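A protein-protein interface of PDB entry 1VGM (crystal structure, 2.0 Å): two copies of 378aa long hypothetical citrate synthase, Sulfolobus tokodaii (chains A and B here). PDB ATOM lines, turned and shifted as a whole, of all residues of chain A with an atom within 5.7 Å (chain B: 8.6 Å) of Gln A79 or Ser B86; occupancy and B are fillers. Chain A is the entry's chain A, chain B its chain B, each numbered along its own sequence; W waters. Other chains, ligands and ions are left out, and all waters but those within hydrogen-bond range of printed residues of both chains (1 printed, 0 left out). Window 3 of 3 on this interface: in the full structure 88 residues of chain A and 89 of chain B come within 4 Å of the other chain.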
ATOM      1  N   PRO A  77     -23.197  12.017  22.000  1.00  0.00           N
ATOM      2  CA  PRO A  77     -23.354  12.215  23.446  1.00  0.00           C
ATOM      3  C   PRO A  77     -22.218  11.525  24.176  1.00  0.00           C
ATOM      4  O   PRO A  77     -21.719  10.492  23.719  1.00  0.00           O
ATOM      5  CB  PRO A  77     -24.704  11.569  23.757  1.00  0.00           C
ATOM      6  CG  PRO A  77     -25.451  11.622  22.452  1.00  0.00           C
ATOM      7  CD  PRO A  77     -24.400  11.418  21.395  1.00  0.00           C
ATOM      8  N   GLU A  78     -21.795  12.091  25.303  1.00  0.00           N
ATOM      9  CA  GLU A  78     -20.649  11.539  26.008  1.00  0.00           C
ATOM     10  C   GLU A  78     -21.017  10.183  26.603  1.00  0.00           C
ATOM     11  O   GLU A  78     -20.144   9.351  26.867  1.00  0.00           O
ATOM     12  CB  GLU A  78     -20.166  12.510  27.095  1.00  0.00           C
ATOM     13  CG  GLU A  78     -21.137  12.764  28.232  1.00  0.00           C
ATOM     14  CD  GLU A  78     -20.572  13.745  29.251  1.00  0.00           C
ATOM     15  OE1 GLU A  78     -21.044  13.744  30.408  1.00  0.00           O
ATOM     16  OE2 GLU A  78     -19.654  14.516  28.890  1.00  0.00           O
ATOM     17  N   GLN A  79     -22.314   9.951  26.796  1.00  0.00           N
ATOM     18  CA  GLN A  79     -22.771   8.646  27.267  1.00  0.00           C
ATOM     19  C   GLN A  79     -22.326   7.535  26.333  1.00  0.00           C
ATOM     20  O   GLN A  79     -22.035   6.427  26.777  1.00  0.00           O
ATOM     21  CB  GLN A  79     -24.297   8.610  27.393  1.00  0.00           C
ATOM     22  CG  GLN A  79     -24.821   9.225  28.678  1.00  0.00           C
ATOM     23  CD  GLN A  79     -25.018  10.723  28.557  1.00  0.00           C
ATOM     24  OE1 GLN A  79     -24.669  11.329  27.538  1.00  0.00           O
ATOM     25  NE2 GLN A  79     -25.581  11.331  29.596  1.00  0.00           N
ATOM     26  N   VAL A  80     -22.281   7.832  25.038  1.00  0.00           N
ATOM     27  CA  VAL A  80     -21.866   6.846  24.044  1.00  0.00           C
ATOM     28  C   VAL A  80     -20.441   6.401  24.324  1.00  0.00           C
ATOM     29  O   VAL A  80     -20.146   5.205  24.389  1.00  0.00           O
ATOM     30  CB  VAL A  80     -21.909   7.426  22.612  1.00  0.00           C
ATOM     31  CG1 VAL A  80     -21.298   6.428  21.630  1.00  0.00           C
ATOM     32  CG2 VAL A  80     -23.335   7.746  22.228  1.00  0.00           C
ATOM     33  N   ILE A  81     -19.556   7.378  24.475  1.00  0.00           N
ATOM     34  CA  ILE A  81     -18.150   7.096  24.717  1.00  0.00           C
ATOM     35  C   ILE A  81     -18.024   6.335  26.036  1.00  0.00           C
ATOM     36  O   ILE A  81     -17.373   5.297  26.113  1.00  0.00           O
ATOM     37  CB  ILE A  81     -17.331   8.413  24.781  1.00  0.00           C
ATOM     38  CG1 ILE A  81     -17.481   9.168  23.460  1.00  0.00           C
ATOM     39  CG2 ILE A  81     -15.852   8.115  25.057  1.00  0.00           C
ATOM     40  CD1 ILE A  81     -16.993   8.394  22.236  1.00  0.00           C
ATOM     41  N   SER A  82     -18.676   6.859  27.064  1.00  0.00           N
ATOM     42  CA  SER A  82     -18.590   6.284  28.392  1.00  0.00           C
ATOM     43  C   SER A  82     -18.970   4.806  28.372  1.00  0.00           C
ATOM     44  O   SER A  82     -18.289   3.970  28.958  1.00  0.00           O
ATOM     45  CB  SER A  82     -19.511   7.049  29.343  1.00  0.00           C
ATOM     46  OG  SER A  82     -19.546   6.421  30.609  1.00  0.00           O
ATOM     47  N   THR A  83     -20.059   4.484  27.687  1.00  0.00           N
ATOM     48  CA  THR A  83     -20.555   3.113  27.663  1.00  0.00           C
ATOM     49  C   THR A  83     -19.704   2.188  26.791  1.00  0.00           C
ATOM     50  O   THR A  83     -19.370   1.077  27.202  1.00  0.00           O
ATOM     51  CB  THR A  83     -22.007   3.073  27.162  1.00  0.00           C
ATOM     52  OG1 THR A  83     -22.845   3.739  28.113  1.00  0.00           O
ATOM     53  CG2 THR A  83     -22.476   1.629  26.978  1.00  0.00           C
ATOM     54  N   ILE A  84     -19.362   2.642  25.591  1.00  0.00           N
ATOM     55  CA  ILE A  84     -18.515   1.869  24.679  1.00  0.00           C
ATOM     56  C   ILE A  84     -17.209   1.469  25.368  1.00  0.00           C
ATOM     57  O   ILE A  84     -16.779   0.307  25.321  1.00  0.00           O
ATOM     58  CB  ILE A  84     -18.189   2.698  23.403  1.00  0.00           C
ATOM     59  CG1 ILE A  84     -19.318   2.553  22.384  1.00  0.00           C
ATOM     60  CG2 ILE A  84     -16.873   2.248  22.791  1.00  0.00           C
ATOM     61  CD1 ILE A  84     -19.121   3.413  21.137  1.00  0.00           C
ATOM     62  N   ILE A 103     -28.307   4.340  22.696  1.00  0.00           N
ATOM     63  CA  ILE A 103     -28.033   5.593  23.388  1.00  0.00           C
ATOM     64  C   ILE A 103     -28.347   6.838  22.548  1.00  0.00           C
ATOM     65  O   ILE A 103     -28.908   7.804  23.067  1.00  0.00           O
ATOM     66  CB  ILE A 103     -26.566   5.640  23.865  1.00  0.00           C
ATOM     67  CG1 ILE A 103     -26.367   4.606  24.978  1.00  0.00           C
ATOM     68  CG2 ILE A 103     -26.212   7.040  24.361  1.00  0.00           C
ATOM     69  CD1 ILE A 103     -24.925   4.357  25.348  1.00  0.00           C
ATOM     70  N   ILE A 107     -31.193   9.756  23.462  1.00  0.00           N
ATOM     71  CA  ILE A 107     -30.789  11.116  23.774  1.00  0.00           C
ATOM     72  C   ILE A 107     -31.255  12.097  22.708  1.00  0.00           C
ATOM     73  O   ILE A 107     -31.770  13.166  23.034  1.00  0.00           O
ATOM     74  CB  ILE A 107     -29.262  11.211  23.951  1.00  0.00           C
ATOM     75  CG1 ILE A 107     -28.850  10.419  25.195  1.00  0.00           C
ATOM     76  CG2 ILE A 107     -28.832  12.677  24.095  1.00  0.00           C
ATOM     77  CD1 ILE A 107     -27.374  10.415  25.472  1.00  0.00           C
ATOM     78  N   GLN B  79     -22.147  -2.386  34.058  1.00  0.00           N
ATOM     79  CA  GLN B  79     -22.286  -1.441  32.951  1.00  0.00           C
ATOM     80  C   GLN B  79     -23.746  -1.158  32.561  1.00  0.00           C
ATOM     81  O   GLN B  79     -24.064  -0.064  32.091  1.00  0.00           O
ATOM     82  CB  GLN B  79     -21.521  -1.950  31.724  1.00  0.00           C
ATOM     83  CG  GLN B  79     -20.033  -2.092  31.950  1.00  0.00           C
ATOM     84  CD  GLN B  79     -19.621  -3.514  32.299  1.00  0.00           C
ATOM     85  OE1 GLN B  79     -20.325  -4.229  33.023  1.00  0.00           O
ATOM     86  NE2 GLN B  79     -18.470  -3.929  31.785  1.00  0.00           N
ATOM     87  N   VAL B  80     -24.632  -2.132  32.756  1.00  0.00           N
ATOM     88  CA  VAL B  80     -26.058  -1.894  32.519  1.00  0.00           C
ATOM     89  C   VAL B  80     -26.605  -0.821  33.457  1.00  0.00           C
ATOM     90  O   VAL B  80     -27.253   0.134  33.021  1.00  0.00           O
ATOM     91  CB  VAL B  80     -26.906  -3.178  32.717  1.00  0.00           C
ATOM     92  CG1 VAL B  80     -28.395  -2.836  32.611  1.00  0.00           C
ATOM     93  CG2 VAL B  80     -26.542  -4.209  31.668  1.00  0.00           C
ATOM     94  N   ILE B  81     -26.351  -0.992  34.747  1.00  0.00           N
ATOM     95  CA  ILE B  81     -26.860  -0.071  35.749  1.00  0.00           C
ATOM     96  C   ILE B  81     -26.205   1.308  35.615  1.00  0.00           C
ATOM     97  O   ILE B  81     -26.897   2.312  35.544  1.00  0.00           O
ATOM     98  CB  ILE B  81     -26.631  -0.628  37.178  1.00  0.00           C
ATOM     99  CG1 ILE B  81     -27.460  -1.899  37.367  1.00  0.00           C
ATOM    100  CG2 ILE B  81     -27.006   0.426  38.235  1.00  0.00           C
ATOM    101  CD1 ILE B  81     -28.972  -1.669  37.332  1.00  0.00           C
ATOM    102  N   SER B  82     -24.878   1.359  35.564  1.00  0.00           N
ATOM    103  CA  SER B  82     -24.195   2.635  35.384  1.00  0.00           C
ATOM    104  C   SER B  82     -24.681   3.377  34.137  1.00  0.00           C
ATOM    105  O   SER B  82     -24.900   4.589  34.178  1.00  0.00           O
ATOM    106  CB  SER B  82     -22.680   2.433  35.301  1.00  0.00           C
ATOM    107  OG  SER B  82     -22.131   2.095  36.568  1.00  0.00           O
ATOM    108  N   THR B  83     -24.853   2.665  33.026  1.00  0.00           N
ATOM    109  CA  THR B  83     -25.320   3.325  31.813  1.00  0.00           C
ATOM    110  C   THR B  83     -26.733   3.849  32.010  1.00  0.00           C
ATOM    111  O   THR B  83     -27.031   4.982  31.644  1.00  0.00           O
ATOM    112  CB  THR B  83     -25.273   2.373  30.593  1.00  0.00           C
ATOM    113  OG1 THR B  83     -23.905   2.163  30.213  1.00  0.00           O
ATOM    114  CG2 THR B  83     -26.030   2.964  29.410  1.00  0.00           C
ATOM    115  N   ILE B  84     -27.609   3.046  32.608  1.00  0.00           N
ATOM    116  CA  ILE B  84     -28.999   3.474  32.799  1.00  0.00           C
ATOM    117  C   ILE B  84     -29.087   4.770  33.625  1.00  0.00           C
ATOM    118  O   ILE B  84     -29.888   5.667  33.322  1.00  0.00           O
ATOM    119  CB  ILE B  84     -29.833   2.373  33.497  1.00  0.00           C
ATOM    120  CG1 ILE B  84     -30.215   1.288  32.488  1.00  0.00           C
ATOM    121  CG2 ILE B  84     -31.109   2.958  34.077  1.00  0.00           C
ATOM    122  CD1 ILE B  84     -30.623  -0.035  33.128  1.00  0.00           C
ATOM    123  N   PHE B  85     -28.257   4.863  34.657  1.00  0.00           N
ATOM    124  CA  PHE B  85     -28.320   5.983  35.586  1.00  0.00           C
ATOM    125  C   PHE B  85     -27.484   7.194  35.147  1.00  0.00           C
ATOM    126  O   PHE B  85     -27.598   8.270  35.723  1.00  0.00           O
ATOM    127  CB  PHE B  85     -27.891   5.512  36.980  1.00  0.00           C
ATOM    128  CG  PHE B  85     -28.977   4.788  37.728  1.00  0.00           C
ATOM    129  CD1 PHE B  85     -29.820   5.477  38.610  1.00  0.00           C
ATOM    130  CD2 PHE B  85     -29.192   3.433  37.515  1.00  0.00           C
ATOM    131  CE1 PHE B  85     -30.857   4.819  39.267  1.00  0.00           C
ATOM    132  CE2 PHE B  85     -30.222   2.768  38.163  1.00  0.00           C
ATOM    133  CZ  PHE B  85     -31.061   3.462  39.041  1.00  0.00           C
ATOM    134  N   SER B  86     -26.658   7.020  34.118  1.00  0.00           N
ATOM    135  CA  SER B  86     -25.965   8.146  33.498  1.00  0.00           C
ATOM    136  C   SER B  86     -26.835   8.833  32.447  1.00  0.00           C
ATOM    137  O   SER B  86     -26.510   9.925  31.992  1.00  0.00           O
ATOM    138  CB  SER B  86     -24.666   7.672  32.832  1.00  0.00           C
ATOM    139  OG  SER B  86     -24.920   7.187  31.518  1.00  0.00           O
ATOM    140  N   MET B  87     -27.935   8.195  32.053  1.00  0.00           N
ATOM    141  CA  MET B  87     -28.772   8.729  30.977  1.00  0.00           C
ATOM    142  C   MET B  87     -29.523   9.951  31.472  1.00  0.00           C
ATOM    143  O   MET B  87     -29.870  10.036  32.651  1.00  0.00           O
ATOM    144  CB  MET B  87     -29.795   7.688  30.497  1.00  0.00           C
ATOM    145  CG  MET B  87     -29.208   6.475  29.796  1.00  0.00           C
ATOM    146  SD  MET B  87     -28.133   6.910  28.412  1.00  0.00           S
ATOM    147  CE  MET B  87     -29.340   7.267  27.146  1.00  0.00           C
ATOM    148  N   PRO B  88     -29.798  10.911  30.573  1.00  0.00           N
ATOM    149  CA  PRO B  88     -30.673  12.031  30.939  1.00  0.00           C
ATOM    150  C   PRO B  88     -32.025  11.513  31.409  1.00  0.00           C
ATOM    151  O   PRO B  88     -32.573  10.580  30.823  1.00  0.00           O
ATOM    152  CB  PRO B  88     -30.788  12.838  29.645  1.00  0.00           C
ATOM    153  CG  PRO B  88     -29.565  12.461  28.857  1.00  0.00           C
ATOM    154  CD  PRO B  88     -29.353  11.005  29.172  1.00  0.00           C
ATOM    155  N   ARG B  89     -32.559  12.123  32.465  1.00  0.00           N
ATOM    156  CA  ARG B  89     -33.683  11.552  33.199  1.00  0.00           C
ATOM    157  C   ARG B  89     -34.992  11.609  32.413  1.00  0.00           C
ATOM    158  O   ARG B  89     -35.985  10.995  32.808  1.00  0.00           O
ATOM    159  CB  ARG B  89     -33.864  12.279  34.533  1.00  0.00           C
ATOM    160  CG  ARG B  89     -32.840  11.913  35.593  1.00  0.00           C
ATOM    161  CD  ARG B  89     -33.095  12.708  36.866  1.00  0.00           C
ATOM    162  NE  ARG B  89     -34.505  12.666  37.245  1.00  0.00           N
ATOM    163  CZ  ARG B  89     -35.058  13.431  38.185  1.00  0.00           C
ATOM    164  NH1 ARG B  89     -34.316  14.302  38.863  1.00  0.00           N
ATOM    165  NH2 ARG B  89     -36.355  13.323  38.448  1.00  0.00           N
ATOM    166  N   CYS B  91     -35.126  10.655  29.218  1.00  0.00           N
ATOM    167  CA  CYS B  91     -35.043   9.676  28.129  1.00  0.00           C
ATOM    168  C   CYS B  91     -36.243   8.739  28.129  1.00  0.00           C
ATOM    169  O   CYS B  91     -36.721   8.321  29.190  1.00  0.00           O
ATOM    170  CB  CYS B  91     -33.765   8.844  28.234  1.00  0.00           C
ATOM    171  SG  CYS B  91     -32.287   9.753  27.833  1.00  0.00           S
ATOM    172  N   MET B  96     -34.137   3.495  26.867  1.00  0.00           N
ATOM    173  CA  MET B  96     -33.218   3.028  27.889  1.00  0.00           C
ATOM    174  C   MET B  96     -33.214   1.506  27.921  1.00  0.00           C
ATOM    175  O   MET B  96     -32.164   0.886  28.106  1.00  0.00           O
ATOM    176  CB  MET B  96     -33.613   3.607  29.252  1.00  0.00           C
ATOM    177  CG  MET B  96     -33.511   5.123  29.300  1.00  0.00           C
ATOM    178  SD  MET B  96     -34.087   5.862  30.843  1.00  0.00           S
ATOM    179  CE  MET B  96     -32.947   5.200  32.025  1.00  0.00           C
ATOM    180  N   THR B  99     -31.314   0.047  24.958  1.00  0.00           N
ATOM    181  CA  THR B  99     -29.902   0.242  25.290  1.00  0.00           C
ATOM    182  C   THR B  99     -29.394  -0.775  26.316  1.00  0.00           C
ATOM    183  O   THR B  99     -28.333  -1.368  26.140  1.00  0.00           O
ATOM    184  CB  THR B  99     -29.645   1.648  25.860  1.00  0.00           C
ATOM    185  OG1 THR B  99     -30.105   2.641  24.928  1.00  0.00           O
ATOM    186  CG2 THR B  99     -28.143   1.833  26.139  1.00  0.00           C
ATOM    187  N   ILE B 103     -26.380  -3.913  25.940  1.00  0.00           N
ATOM    188  CA  ILE B 103     -25.276  -4.217  26.859  1.00  0.00           C
ATOM    189  C   ILE B 103     -25.320  -5.662  27.388  1.00  0.00           C
ATOM    190  O   ILE B 103     -24.283  -6.319  27.509  1.00  0.00           O
ATOM    191  CB  ILE B 103     -25.273  -3.222  28.064  1.00  0.00           C
ATOM    192  CG1 ILE B 103     -24.898  -1.820  27.570  1.00  0.00           C
ATOM    193  CG2 ILE B 103     -24.283  -3.662  29.137  1.00  0.00           C
ATOM    194  CD1 ILE B 103     -25.310  -0.708  28.505  1.00  0.00           C
ATOM    195  N   ALA B 138     -34.050   5.415  37.949  1.00  0.00           N
ATOM    196  CA  ALA B 138     -33.196   6.362  37.241  1.00  0.00           C
ATOM    197  C   ALA B 138     -33.942   7.630  36.826  1.00  0.00           C
ATOM    198  O   ALA B 138     -33.494   8.738  37.110  1.00  0.00           O
ATOM    199  CB  ALA B 138     -32.589   5.691  36.010  1.00  0.00           C
HETATM  200  O   HOH W   1     -22.980   6.182  29.840  1.00  0.00           O
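O of Ser B86 lies within hydrogen-bond range of NE2 of Gln A79.
OG1 of Thr A83 lies within hydrogen-bond range of OG1 of Thr B83 (2.8 Å).
The backbone NH (N) of Ile A103 is in hydrogen-bond range of the side-chain hydroxyl (OG1) of Thr B99.
The backbone carbonyl oxygen (O) of Gln A79 is in hydrogen-bond range of the side-chain hydroxyl (OG1) of Thr A83.
The backbone carbonyl oxygen of Gln B79 is in hydrogen-bond range of the side-chain hydroxyl of Thr B83 (2.9 Å).
The side-chain hydroxyl of Ser B86 sits at hydrogen-bond distance from the backbone carbonyl oxygen of Thr B83 (3.1 Å).
The backbone carbonyl oxygen of Pro B88 lies within hydrogen-bond range of the side-chain sulfur of Cys B91, at 3.1 Å.
Pro B88 touches Gln A79 (CD to NE2, 3.8 Å).
CG2 of Thr A83 touches CD1 of Ile B103, at 3.98 Å.
CG1 of Ile A107 touches CE of Met B87, 3.7 Å away.
Gln A79 touches just these residues of chain B: Ser B86 and Pro B88.
Printed residues of chain A within 4 Å of Ser B86: Gln A79 (2.9 Å).
Of the printed residues of chain A, Thr B99 touches Ile A103.
Of the printed residues of chain A, Met B87 touches Ile A107.
Of the printed residues of chain A, Thr B83 touches Thr A83.
Ile B84 touches none of the printed residues of chain A.
The nearest residue of chain B that does not touch Gln A79 is Met B87 (4.05 Å).
The nearest residue of chain A that does not touch Ser B86 is Thr A83 (5.3 Å).
Of the 10 printed residues of chain A, 4 touch a printed residue of chain B.
Printed residues of chain A that touch a printed residue of chain B: Gln A79, Thr A83, Ile A103 and Ile A107.
Hydrophobic or aromatic side chains of chain A within 4 Å of the printed part of chain B: Ile A103 and Ile A107.
Printed residues of chain B that touch a printed residue of chain A: Thr B83, Ser B86, Met B87, Pro B88, Thr B99 and Ile B103.
Hydrophobic or aromatic side chains of chain B within 4 Å of the printed part of chain A: Met B87, Pro B88 and Ile B103.
Along chain B the printed residues that touch a printed residue of chain A span positions 83 to 103.
Among the printed residues, 6 pairs touch across the chains.
Thr B83 touches its own counterpart, Thr A83.
Thr A83 touches Ile B103, but with the chains exchanged Ile A103 does not touch Thr B83 (4.4 Å).
Positions printed for both chains: 79, 80, 81, 82, 83, 84 and 103.
Of the 6 pairs that touch across the chains among the printed residues, 1 has its exchanged pair printed and touching as well.
Water W1 lies within hydrogen-bond range of the side-chain hydroxyl of Ser B86, the side-chain hydroxyl of Thr A83 and the backbone carbonyl oxygen of Gln A79.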
